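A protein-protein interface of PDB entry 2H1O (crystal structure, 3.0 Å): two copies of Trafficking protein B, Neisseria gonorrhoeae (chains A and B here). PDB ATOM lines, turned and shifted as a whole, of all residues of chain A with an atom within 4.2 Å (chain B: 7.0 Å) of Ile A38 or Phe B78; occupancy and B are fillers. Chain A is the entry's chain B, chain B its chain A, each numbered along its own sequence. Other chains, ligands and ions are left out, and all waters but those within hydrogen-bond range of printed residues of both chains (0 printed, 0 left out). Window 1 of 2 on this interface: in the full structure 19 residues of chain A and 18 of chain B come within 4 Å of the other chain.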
ATOM      1  N   SER A  36       2.714 -18.922  13.875  1.00  0.00           N
ATOM      2  CA  SER A  36       2.549 -17.579  14.346  1.00  0.00           C
ATOM      3  C   SER A  36       3.329 -17.451  15.623  1.00  0.00           C
ATOM      4  O   SER A  36       3.374 -18.384  16.415  1.00  0.00           O
ATOM      5  CB  SER A  36       1.098 -17.301  14.646  1.00  0.00           C
ATOM      6  OG  SER A  36       1.027 -16.251  15.582  1.00  0.00           O
ATOM      7  N   ALA A  37       3.960 -16.303  15.822  1.00  0.00           N
ATOM      8  CA  ALA A  37       4.677 -16.076  17.052  1.00  0.00           C
ATOM      9  C   ALA A  37       3.674 -16.366  18.179  1.00  0.00           C
ATOM     10  O   ALA A  37       4.021 -17.009  19.171  1.00  0.00           O
ATOM     11  CB  ALA A  37       5.136 -14.651  17.115  1.00  0.00           C
ATOM     12  N   ILE A  38       2.431 -15.905  18.018  1.00  0.00           N
ATOM     13  CA  ILE A  38       1.390 -16.139  19.021  1.00  0.00           C
ATOM     14  C   ILE A  38       1.272 -17.638  19.288  1.00  0.00           C
ATOM     15  O   ILE A  38       1.070 -18.068  20.428  1.00  0.00           O
ATOM     16  CB  ILE A  38       0.001 -15.630  18.554  1.00  0.00           C
ATOM     17  CG1 ILE A  38       0.051 -14.134  18.286  1.00  0.00           C
ATOM     18  CG2 ILE A  38      -1.046 -15.898  19.612  1.00  0.00           C
ATOM     19  CD1 ILE A  38       0.406 -13.313  19.493  1.00  0.00           C
ATOM     20  N   THR A  39       1.396 -18.441  18.235  1.00  0.00           N
ATOM     21  CA  THR A  39       1.286 -19.881  18.394  1.00  0.00           C
ATOM     22  C   THR A  39       2.520 -20.462  19.058  1.00  0.00           C
ATOM     23  O   THR A  39       2.412 -21.379  19.874  1.00  0.00           O
ATOM     24  CB  THR A  39       1.076 -20.585  17.056  1.00  0.00           C
ATOM     25  OG1 THR A  39      -0.107 -20.076  16.432  1.00  0.00           O
ATOM     26  CG2 THR A  39       0.920 -22.084  17.272  1.00  0.00           C
ATOM     27  N   VAL A  40       3.693 -19.946  18.708  1.00  0.00           N
ATOM     28  CA  VAL A  40       4.927 -20.439  19.310  1.00  0.00           C
ATOM     29  C   VAL A  40       4.901 -20.071  20.784  1.00  0.00           C
ATOM     30  O   VAL A  40       5.322 -20.854  21.629  1.00  0.00           O
ATOM     31  CB  VAL A  40       6.180 -19.828  18.650  1.00  0.00           C
ATOM     32  CG1 VAL A  40       7.413 -20.265  19.391  1.00  0.00           C
ATOM     33  CG2 VAL A  40       6.284 -20.284  17.215  1.00  0.00           C
ATOM     34  N   ALA A  41       4.389 -18.881  21.086  1.00  0.00           N
ATOM     35  CA  ALA A  41       4.281 -18.411  22.462  1.00  0.00           C
ATOM     36  C   ALA A  41       3.359 -19.318  23.269  1.00  0.00           C
ATOM     37  O   ALA A  41       3.580 -19.546  24.446  1.00  0.00           O
ATOM     38  CB  ALA A  41       3.755 -16.990  22.487  1.00  0.00           C
ATOM     39  N   GLU A  42       2.314 -19.832  22.635  1.00  0.00           N
ATOM     40  CA  GLU A  42       1.393 -20.720  23.326  1.00  0.00           C
ATOM     41  C   GLU A  42       2.087 -22.074  23.597  1.00  0.00           C
ATOM     42  O   GLU A  42       1.918 -22.658  24.658  1.00  0.00           O
ATOM     43  CB  GLU A  42       0.134 -20.915  22.475  1.00  0.00           C
ATOM     44  CG  GLU A  42      -1.207 -20.690  23.203  1.00  0.00           C
ATOM     45  CD  GLU A  42      -2.444 -21.025  22.315  1.00  0.00           C
ATOM     46  OE1 GLU A  42      -2.621 -20.397  21.233  1.00  0.00           O
ATOM     47  OE2 GLU A  42      -3.241 -21.921  22.704  1.00  0.00           O
ATOM     48  N   PRO A  77       5.501 -12.801  12.746  1.00  0.00           N
ATOM     49  CA  PRO A  77       5.258 -11.878  13.853  1.00  0.00           C
ATOM     50  C   PRO A  77       3.907 -11.191  13.718  1.00  0.00           C
ATOM     51  O   PRO A  77       3.387 -11.026  12.610  1.00  0.00           O
ATOM     52  CB  PRO A  77       6.387 -10.887  13.691  1.00  0.00           C
ATOM     53  CG  PRO A  77       6.368 -10.689  12.204  1.00  0.00           C
ATOM     54  CD  PRO A  77       6.247 -12.119  11.674  1.00  0.00           C
ATOM     55  N   PHE A  78       3.349 -10.780  14.849  1.00  0.00           N
ATOM     56  CA  PHE A  78       2.079 -10.084  14.845  1.00  0.00           C
ATOM     57  C   PHE A  78       2.436  -8.609  14.930  1.00  0.00           C
ATOM     58  O   PHE A  78       2.755  -8.114  15.999  1.00  0.00           O
ATOM     59  CB  PHE A  78       1.254 -10.491  16.060  1.00  0.00           C
ATOM     60  CG  PHE A  78      -0.099  -9.866  16.101  1.00  0.00           C
ATOM     61  CD1 PHE A  78      -1.141 -10.382  15.346  1.00  0.00           C
ATOM     62  CD2 PHE A  78      -0.333  -8.742  16.881  1.00  0.00           C
ATOM     63  CE1 PHE A  78      -2.401  -9.789  15.366  1.00  0.00           C
ATOM     64  CE2 PHE A  78      -1.593  -8.136  16.909  1.00  0.00           C
ATOM     65  CZ  PHE A  78      -2.626  -8.661  16.151  1.00  0.00           C
ATOM     66  N   TYR A 106      -5.924 -13.671  15.920  1.00  0.00           N
ATOM     67  CA  TYR A 106      -4.498 -13.427  15.724  1.00  0.00           C
ATOM     68  C   TYR A 106      -3.927 -14.305  14.616  1.00  0.00           C
ATOM     69  O   TYR A 106      -3.244 -13.824  13.713  1.00  0.00           O
ATOM     70  CB  TYR A 106      -3.741 -13.715  17.015  1.00  0.00           C
ATOM     71  CG  TYR A 106      -4.108 -12.829  18.171  1.00  0.00           C
ATOM     72  CD1 TYR A 106      -4.290 -13.370  19.445  1.00  0.00           C
ATOM     73  CD2 TYR A 106      -4.241 -11.450  18.010  1.00  0.00           C
ATOM     74  CE1 TYR A 106      -4.595 -12.557  20.540  1.00  0.00           C
ATOM     75  CE2 TYR A 106      -4.548 -10.627  19.098  1.00  0.00           C
ATOM     76  CZ  TYR A 106      -4.722 -11.190  20.359  1.00  0.00           C
ATOM     77  OH  TYR A 106      -5.012 -10.405  21.448  1.00  0.00           O
ATOM     78  N   SER B  36       2.248  -1.475  21.751  1.00  0.00           N
ATOM     79  CA  SER B  36       2.417  -2.854  21.322  1.00  0.00           C
ATOM     80  C   SER B  36       1.452  -3.105  20.164  1.00  0.00           C
ATOM     81  O   SER B  36       0.341  -2.566  20.138  1.00  0.00           O
ATOM     82  CB  SER B  36       2.091  -3.837  22.442  1.00  0.00           C
ATOM     83  OG  SER B  36       2.159  -5.176  21.959  1.00  0.00           O
ATOM     84  N   ALA B  37       1.875  -3.916  19.201  1.00  0.00           N
ATOM     85  CA  ALA B  37       1.018  -4.247  18.072  1.00  0.00           C
ATOM     86  C   ALA B  37      -0.305  -4.724  18.661  1.00  0.00           C
ATOM     87  O   ALA B  37      -1.372  -4.355  18.173  1.00  0.00           O
ATOM     88  CB  ALA B  37       1.649  -5.345  17.233  1.00  0.00           C
ATOM     89  N   ILE B  38      -0.219  -5.531  19.722  1.00  0.00           N
ATOM     90  CA  ILE B  38      -1.401  -6.047  20.403  1.00  0.00           C
ATOM     91  C   ILE B  38      -2.297  -4.884  20.764  1.00  0.00           C
ATOM     92  O   ILE B  38      -3.494  -4.904  20.486  1.00  0.00           O
ATOM     93  CB  ILE B  38      -1.060  -6.761  21.714  1.00  0.00           C
ATOM     94  CG1 ILE B  38      -0.173  -7.970  21.447  1.00  0.00           C
ATOM     95  CG2 ILE B  38      -2.333  -7.229  22.389  1.00  0.00           C
ATOM     96  CD1 ILE B  38      -0.845  -9.031  20.593  1.00  0.00           C
ATOM     97  N   LEU B  76       5.632  -1.944  18.688  1.00  0.00           N
ATOM     98  CA  LEU B  76       6.310  -3.199  18.924  1.00  0.00           C
ATOM     99  C   LEU B  76       5.572  -4.484  18.624  1.00  0.00           C
ATOM    100  O   LEU B  76       4.571  -4.821  19.264  1.00  0.00           O
ATOM    101  CB  LEU B  76       6.806  -3.227  20.372  1.00  0.00           C
ATOM    102  CG  LEU B  76       7.581  -1.974  20.803  1.00  0.00           C
ATOM    103  CD1 LEU B  76       7.941  -2.088  22.274  1.00  0.00           C
ATOM    104  CD2 LEU B  76       8.825  -1.803  19.934  1.00  0.00           C
ATOM    105  N   PRO B  77       6.101  -5.251  17.661  1.00  0.00           N
ATOM    106  CA  PRO B  77       5.558  -6.528  17.209  1.00  0.00           C
ATOM    107  C   PRO B  77       5.786  -7.615  18.223  1.00  0.00           C
ATOM    108  O   PRO B  77       6.737  -7.565  18.990  1.00  0.00           O
ATOM    109  CB  PRO B  77       6.354  -6.799  15.954  1.00  0.00           C
ATOM    110  CG  PRO B  77       7.691  -6.265  16.323  1.00  0.00           C
ATOM    111  CD  PRO B  77       7.339  -4.935  16.926  1.00  0.00           C
ATOM    112  N   PHE B  78       4.910  -8.604  18.214  1.00  0.00           N
ATOM    113  CA  PHE B  78       5.062  -9.731  19.107  1.00  0.00           C
ATOM    114  C   PHE B  78       5.771 -10.808  18.286  1.00  0.00           C
ATOM    115  O   PHE B  78       5.131 -11.695  17.727  1.00  0.00           O
ATOM    116  CB  PHE B  78       3.714 -10.246  19.550  1.00  0.00           C
ATOM    117  CG  PHE B  78       3.803 -11.331  20.561  1.00  0.00           C
ATOM    118  CD1 PHE B  78       3.854 -11.028  21.920  1.00  0.00           C
ATOM    119  CD2 PHE B  78       3.842 -12.666  20.165  1.00  0.00           C
ATOM    120  CE1 PHE B  78       3.937 -12.040  22.872  1.00  0.00           C
ATOM    121  CE2 PHE B  78       3.927 -13.688  21.106  1.00  0.00           C
ATOM    122  CZ  PHE B  78       3.973 -13.375  22.462  1.00  0.00           C
ATOM    123  N   ASP B  79       7.095 -10.701  18.209  1.00  0.00           N
ATOM    124  CA  ASP B  79       7.938 -11.625  17.463  1.00  0.00           C
ATOM    125  C   ASP B  79       8.334 -12.862  18.278  1.00  0.00           C
ATOM    126  O   ASP B  79       8.087 -12.918  19.484  1.00  0.00           O
ATOM    127  CB  ASP B  79       9.193 -10.881  17.005  1.00  0.00           C
ATOM    128  CG  ASP B  79       9.885 -10.131  18.149  1.00  0.00           C
ATOM    129  OD1 ASP B  79      10.120 -10.752  19.212  1.00  0.00           O
ATOM    130  OD2 ASP B  79      10.204  -8.924  17.990  1.00  0.00           O
ATOM    131  N   GLU B  80       8.958 -13.843  17.618  1.00  0.00           N
ATOM    132  CA  GLU B  80       9.397 -15.094  18.267  1.00  0.00           C
ATOM    133  C   GLU B  80      10.187 -14.892  19.578  1.00  0.00           C
ATOM    134  O   GLU B  80       9.943 -15.578  20.584  1.00  0.00           O
ATOM    135  CB  GLU B  80      10.223 -15.938  17.277  1.00  0.00           C
ATOM    136  CG  GLU B  80      10.833 -17.229  17.846  1.00  0.00           C
ATOM    137  CD  GLU B  80      12.092 -16.968  18.674  1.00  0.00           C
ATOM    138  OE1 GLU B  80      12.954 -16.199  18.196  1.00  0.00           O
ATOM    139  OE2 GLU B  80      12.229 -17.523  19.792  1.00  0.00           O
ATOM    140  N   PRO B  81      11.166 -13.971  19.575  1.00  0.00           N
ATOM    141  CA  PRO B  81      11.920 -13.757  20.808  1.00  0.00           C
ATOM    142  C   PRO B  81      10.939 -13.433  21.926  1.00  0.00           C
ATOM    143  O   PRO B  81      10.884 -14.121  22.949  1.00  0.00           O
ATOM    144  CB  PRO B  81      12.790 -12.555  20.472  1.00  0.00           C
ATOM    145  CG  PRO B  81      13.046 -12.736  19.028  1.00  0.00           C
ATOM    146  CD  PRO B  81      11.703 -13.144  18.481  1.00  0.00           C
ATOM    147  N   VAL B  82      10.140 -12.393  21.715  1.00  0.00           N
ATOM    148  CA  VAL B  82       9.206 -11.995  22.737  1.00  0.00           C
ATOM    149  C   VAL B  82       8.409 -13.162  23.255  1.00  0.00           C
ATOM    150  O   VAL B  82       8.043 -13.198  24.427  1.00  0.00           O
ATOM    151  CB  VAL B  82       8.225 -10.943  22.249  1.00  0.00           C
ATOM    152  CG1 VAL B  82       7.397 -10.455  23.420  1.00  0.00           C
ATOM    153  CG2 VAL B  82       8.973  -9.797  21.617  1.00  0.00           C
ATOM    154  N   ALA B  83       8.140 -14.129  22.398  1.00  0.00           N
ATOM    155  CA  ALA B  83       7.350 -15.253  22.843  1.00  0.00           C
ATOM    156  C   ALA B  83       8.030 -15.983  23.985  1.00  0.00           C
ATOM    157  O   ALA B  83       7.402 -16.308  24.988  1.00  0.00           O
ATOM    158  CB  ALA B  83       7.089 -16.200  21.686  1.00  0.00           C
ATOM    159  N   ALA B  84       9.320 -16.238  23.833  1.00  0.00           N
ATOM    160  CA  ALA B  84      10.078 -16.948  24.857  1.00  0.00           C
ATOM    161  C   ALA B  84       9.913 -16.252  26.193  1.00  0.00           C
ATOM    162  O   ALA B  84       9.691 -16.900  27.221  1.00  0.00           O
ATOM    163  CB  ALA B  84      11.555 -17.002  24.477  1.00  0.00           C
ATOM    164  N   TYR B  86       7.493 -14.201  27.089  1.00  0.00           N
ATOM    165  CA  TYR B  86       6.099 -14.390  27.464  1.00  0.00           C
ATOM    166  C   TYR B  86       5.939 -15.716  28.195  1.00  0.00           C
ATOM    167  O   TYR B  86       5.294 -15.791  29.238  1.00  0.00           O
ATOM    168  CB  TYR B  86       5.234 -14.400  26.209  1.00  0.00           C
ATOM    169  CG  TYR B  86       3.854 -14.976  26.396  1.00  0.00           C
ATOM    170  CD1 TYR B  86       2.814 -14.200  26.883  1.00  0.00           C
ATOM    171  CD2 TYR B  86       3.588 -16.304  26.053  1.00  0.00           C
ATOM    172  CE1 TYR B  86       1.532 -14.726  27.020  1.00  0.00           C
ATOM    173  CE2 TYR B  86       2.316 -16.844  26.187  1.00  0.00           C
ATOM    174  CZ  TYR B  86       1.289 -16.049  26.668  1.00  0.00           C
ATOM    175  OH  TYR B  86       0.017 -16.570  26.784  1.00  0.00           O
ATOM    176  N   ALA B  87       6.535 -16.763  27.638  1.00  0.00           N
ATOM    177  CA  ALA B  87       6.442 -18.079  28.242  1.00  0.00           C
ATOM    178  C   ALA B  87       6.874 -18.060  29.702  1.00  0.00           C
ATOM    179  O   ALA B  87       6.235 -18.690  30.548  1.00  0.00           O
ATOM    180  CB  ALA B  87       7.287 -19.077  27.457  1.00  0.00           C
ATOM    181  N   ALA B 102      -3.279 -13.878  29.125  1.00  0.00           N
ATOM    182  CA  ALA B 102      -2.463 -13.846  27.920  1.00  0.00           C
ATOM    183  C   ALA B 102      -2.244 -12.438  27.357  1.00  0.00           C
ATOM    184  O   ALA B 102      -1.116 -12.018  27.138  1.00  0.00           O
ATOM    185  CB  ALA B 102      -3.084 -14.737  26.864  1.00  0.00           C
ATOM    186  N   GLY B 105       0.030 -10.685  29.242  1.00  0.00           N
ATOM    187  CA  GLY B 105       1.334 -11.308  29.168  1.00  0.00           C
ATOM    188  C   GLY B 105       2.070 -10.849  27.924  1.00  0.00           C
ATOM    189  O   GLY B 105       3.289 -10.692  27.932  1.00  0.00           O
ATOM    190  N   TYR B 106       1.324 -10.635  26.847  1.00  0.00           N
ATOM    191  CA  TYR B 106       1.918 -10.206  25.591  1.00  0.00           C
ATOM    192  C   TYR B 106       2.546  -8.844  25.825  1.00  0.00           C
ATOM    193  O   TYR B 106       3.718  -8.622  25.519  1.00  0.00           O
ATOM    194  CB  TYR B 106       0.842 -10.139  24.481  1.00  0.00           C
ATOM    195  CG  TYR B 106       0.242 -11.494  24.093  1.00  0.00           C
ATOM    196  CD1 TYR B 106      -1.039 -11.587  23.531  1.00  0.00           C
ATOM    197  CD2 TYR B 106       0.944 -12.678  24.312  1.00  0.00           C
ATOM    198  CE1 TYR B 106      -1.603 -12.822  23.205  1.00  0.00           C
ATOM    199  CE2 TYR B 106       0.388 -13.918  23.991  1.00  0.00           C
ATOM    200  CZ  TYR B 106      -0.881 -13.985  23.439  1.00  0.00           C
ATOM    201  OH  TYR B 106      -1.406 -15.222  23.132  1.00  0.00           O
ATOM    202  N   ILE B 107       1.763  -7.942  26.401  1.00  0.00           N
ATOM    203  CA  ILE B 107       2.234  -6.595  26.686  1.00  0.00           C
ATOM    204  C   ILE B 107       3.440  -6.616  27.623  1.00  0.00           C
ATOM    205  O   ILE B 107       4.464  -6.011  27.326  1.00  0.00           O
ATOM    206  CB  ILE B 107       1.090  -5.715  27.298  1.00  0.00           C
ATOM    207  CG1 ILE B 107       0.202  -5.132  26.185  1.00  0.00           C
ATOM    208  CG2 ILE B 107       1.678  -4.575  28.108  1.00  0.00           C
ATOM    209  CD1 ILE B 107      -0.541  -6.164  25.358  1.00  0.00           C
ATOM    210  N   ALA B 109       5.505  -9.135  28.469  1.00  0.00           N
ATOM    211  CA  ALA B 109       6.585  -9.771  27.755  1.00  0.00           C
ATOM    212  C   ALA B 109       7.219  -8.793  26.786  1.00  0.00           C
ATOM    213  O   ALA B 109       8.436  -8.655  26.764  1.00  0.00           O
ATOM    214  CB  ALA B 109       6.072 -10.992  27.020  1.00  0.00           C
ATOM    215  N   THR B 110       6.408  -8.111  25.986  1.00  0.00           N
ATOM    216  CA  THR B 110       6.966  -7.152  25.040  1.00  0.00           C
ATOM    217  C   THR B 110       7.814  -6.134  25.806  1.00  0.00           C
ATOM    218  O   THR B 110       9.018  -6.024  25.587  1.00  0.00           O
ATOM    219  CB  THR B 110       5.865  -6.410  24.266  1.00  0.00           C
ATOM    220  OG1 THR B 110       5.138  -7.340  23.459  1.00  0.00           O
ATOM    221  CG2 THR B 110       6.468  -5.358  23.361  1.00  0.00           C
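Hydrophobic or aromatic side chains of chain B within 4 Å of the printed part of chain A: Ala B37, Ile B38, Pro B77, Phe B78, Ala B83, Tyr B86 and Tyr B106. Of the 10 printed residues of chain A, 5 touch a printed residue of chain B. Among the printed residues, 13 pairs touch across the chains. Among the printed residues, no Asp or Glu carboxylate lies within 4 Å of a Lys or Arg side-chain nitrogen of the other chain.
OG of Ser B36 lies close to N of Ile B38, 3.3 Å away. The backbone carbonyl oxygen (O) of Leu B76 is in hydrogen-bond range of the backbone NH (N) of Ala B37 (2.8 Å). The side-chain carboxylate of Asp B79 lies close to the backbone NH of Val B82 (3.0 Å). The side-chain hydroxyl (OG1) of Thr B110 sits at hydrogen-bond distance from the backbone carbonyl oxygen (O) of Tyr B106, at 2.8 Å. N of Ile A38 lies within hydrogen-bond range of OG of Ser A36 (2.8 Å).
Ala A37 touches Phe B78 (CB to O, 3.0 Å). Ala A37 touches Glu B80. Ile A38 touches Tyr B106 (CG2 to OH, 3.6 Å). Phe B78 touches Ala A41. CB of Ala B83 touches CB of Ala A41 (3.5 Å). Ala A41 touches Tyr B86 (O to CE2, 3.5 Å). CA of Pro A77 touches O of Phe B78, at 3.9 Å. O of Phe A78 touches CB of Ala B37, at 3.2 Å. CD1 of Ile B38 touches CD2 of Phe A78, 3.8 Å away. Pro B77 touches Phe A78.
Ile A38 touches just these residues of chain B: Phe B78 (3.6 Å) and Tyr B106 (3.6 Å). Of the printed residues of chain A, Phe B78 touches Ala A37, Ile A38, Ala A41, Pro A77 and Phe A78. Printed residues of chain B within 4 Å of Ala A37: Phe B78 (3.0 Å), Asp B79 (3.8 Å) and Glu B80 (3.9 Å). Of the printed residues of chain A, Ile B38 touches Phe A78 (3.8 Å). Of the printed residues of chain A, Ala B83 touches Ala A41 (3.5 Å). Ala B109 touches none of the printed residues of chain A. The nearest residue of chain B that does not touch Ile A38 is Ile B38 (4.6 Å).
The backbone NH (N) of Phe B78 is in hydrogen-bond range of the backbone carbonyl oxygen (O) of Phe A78.
Ala A37 touches Phe B78, and with the chains exchanged Phe A78 touches Ala B37. Ile A38 touches Phe B78, and with the chains exchanged Phe A78 touches Ile B38. Pro A77 touches Phe B78, and with the chains exchanged Phe A78 touches Pro B77. Phe A78 touches its own counterpart, Phe B78. 6 positions are printed for both chains. Of the 13 pairs that touch across the chains among the printed residues, 7 have their exchanged pair printed and touching as well.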
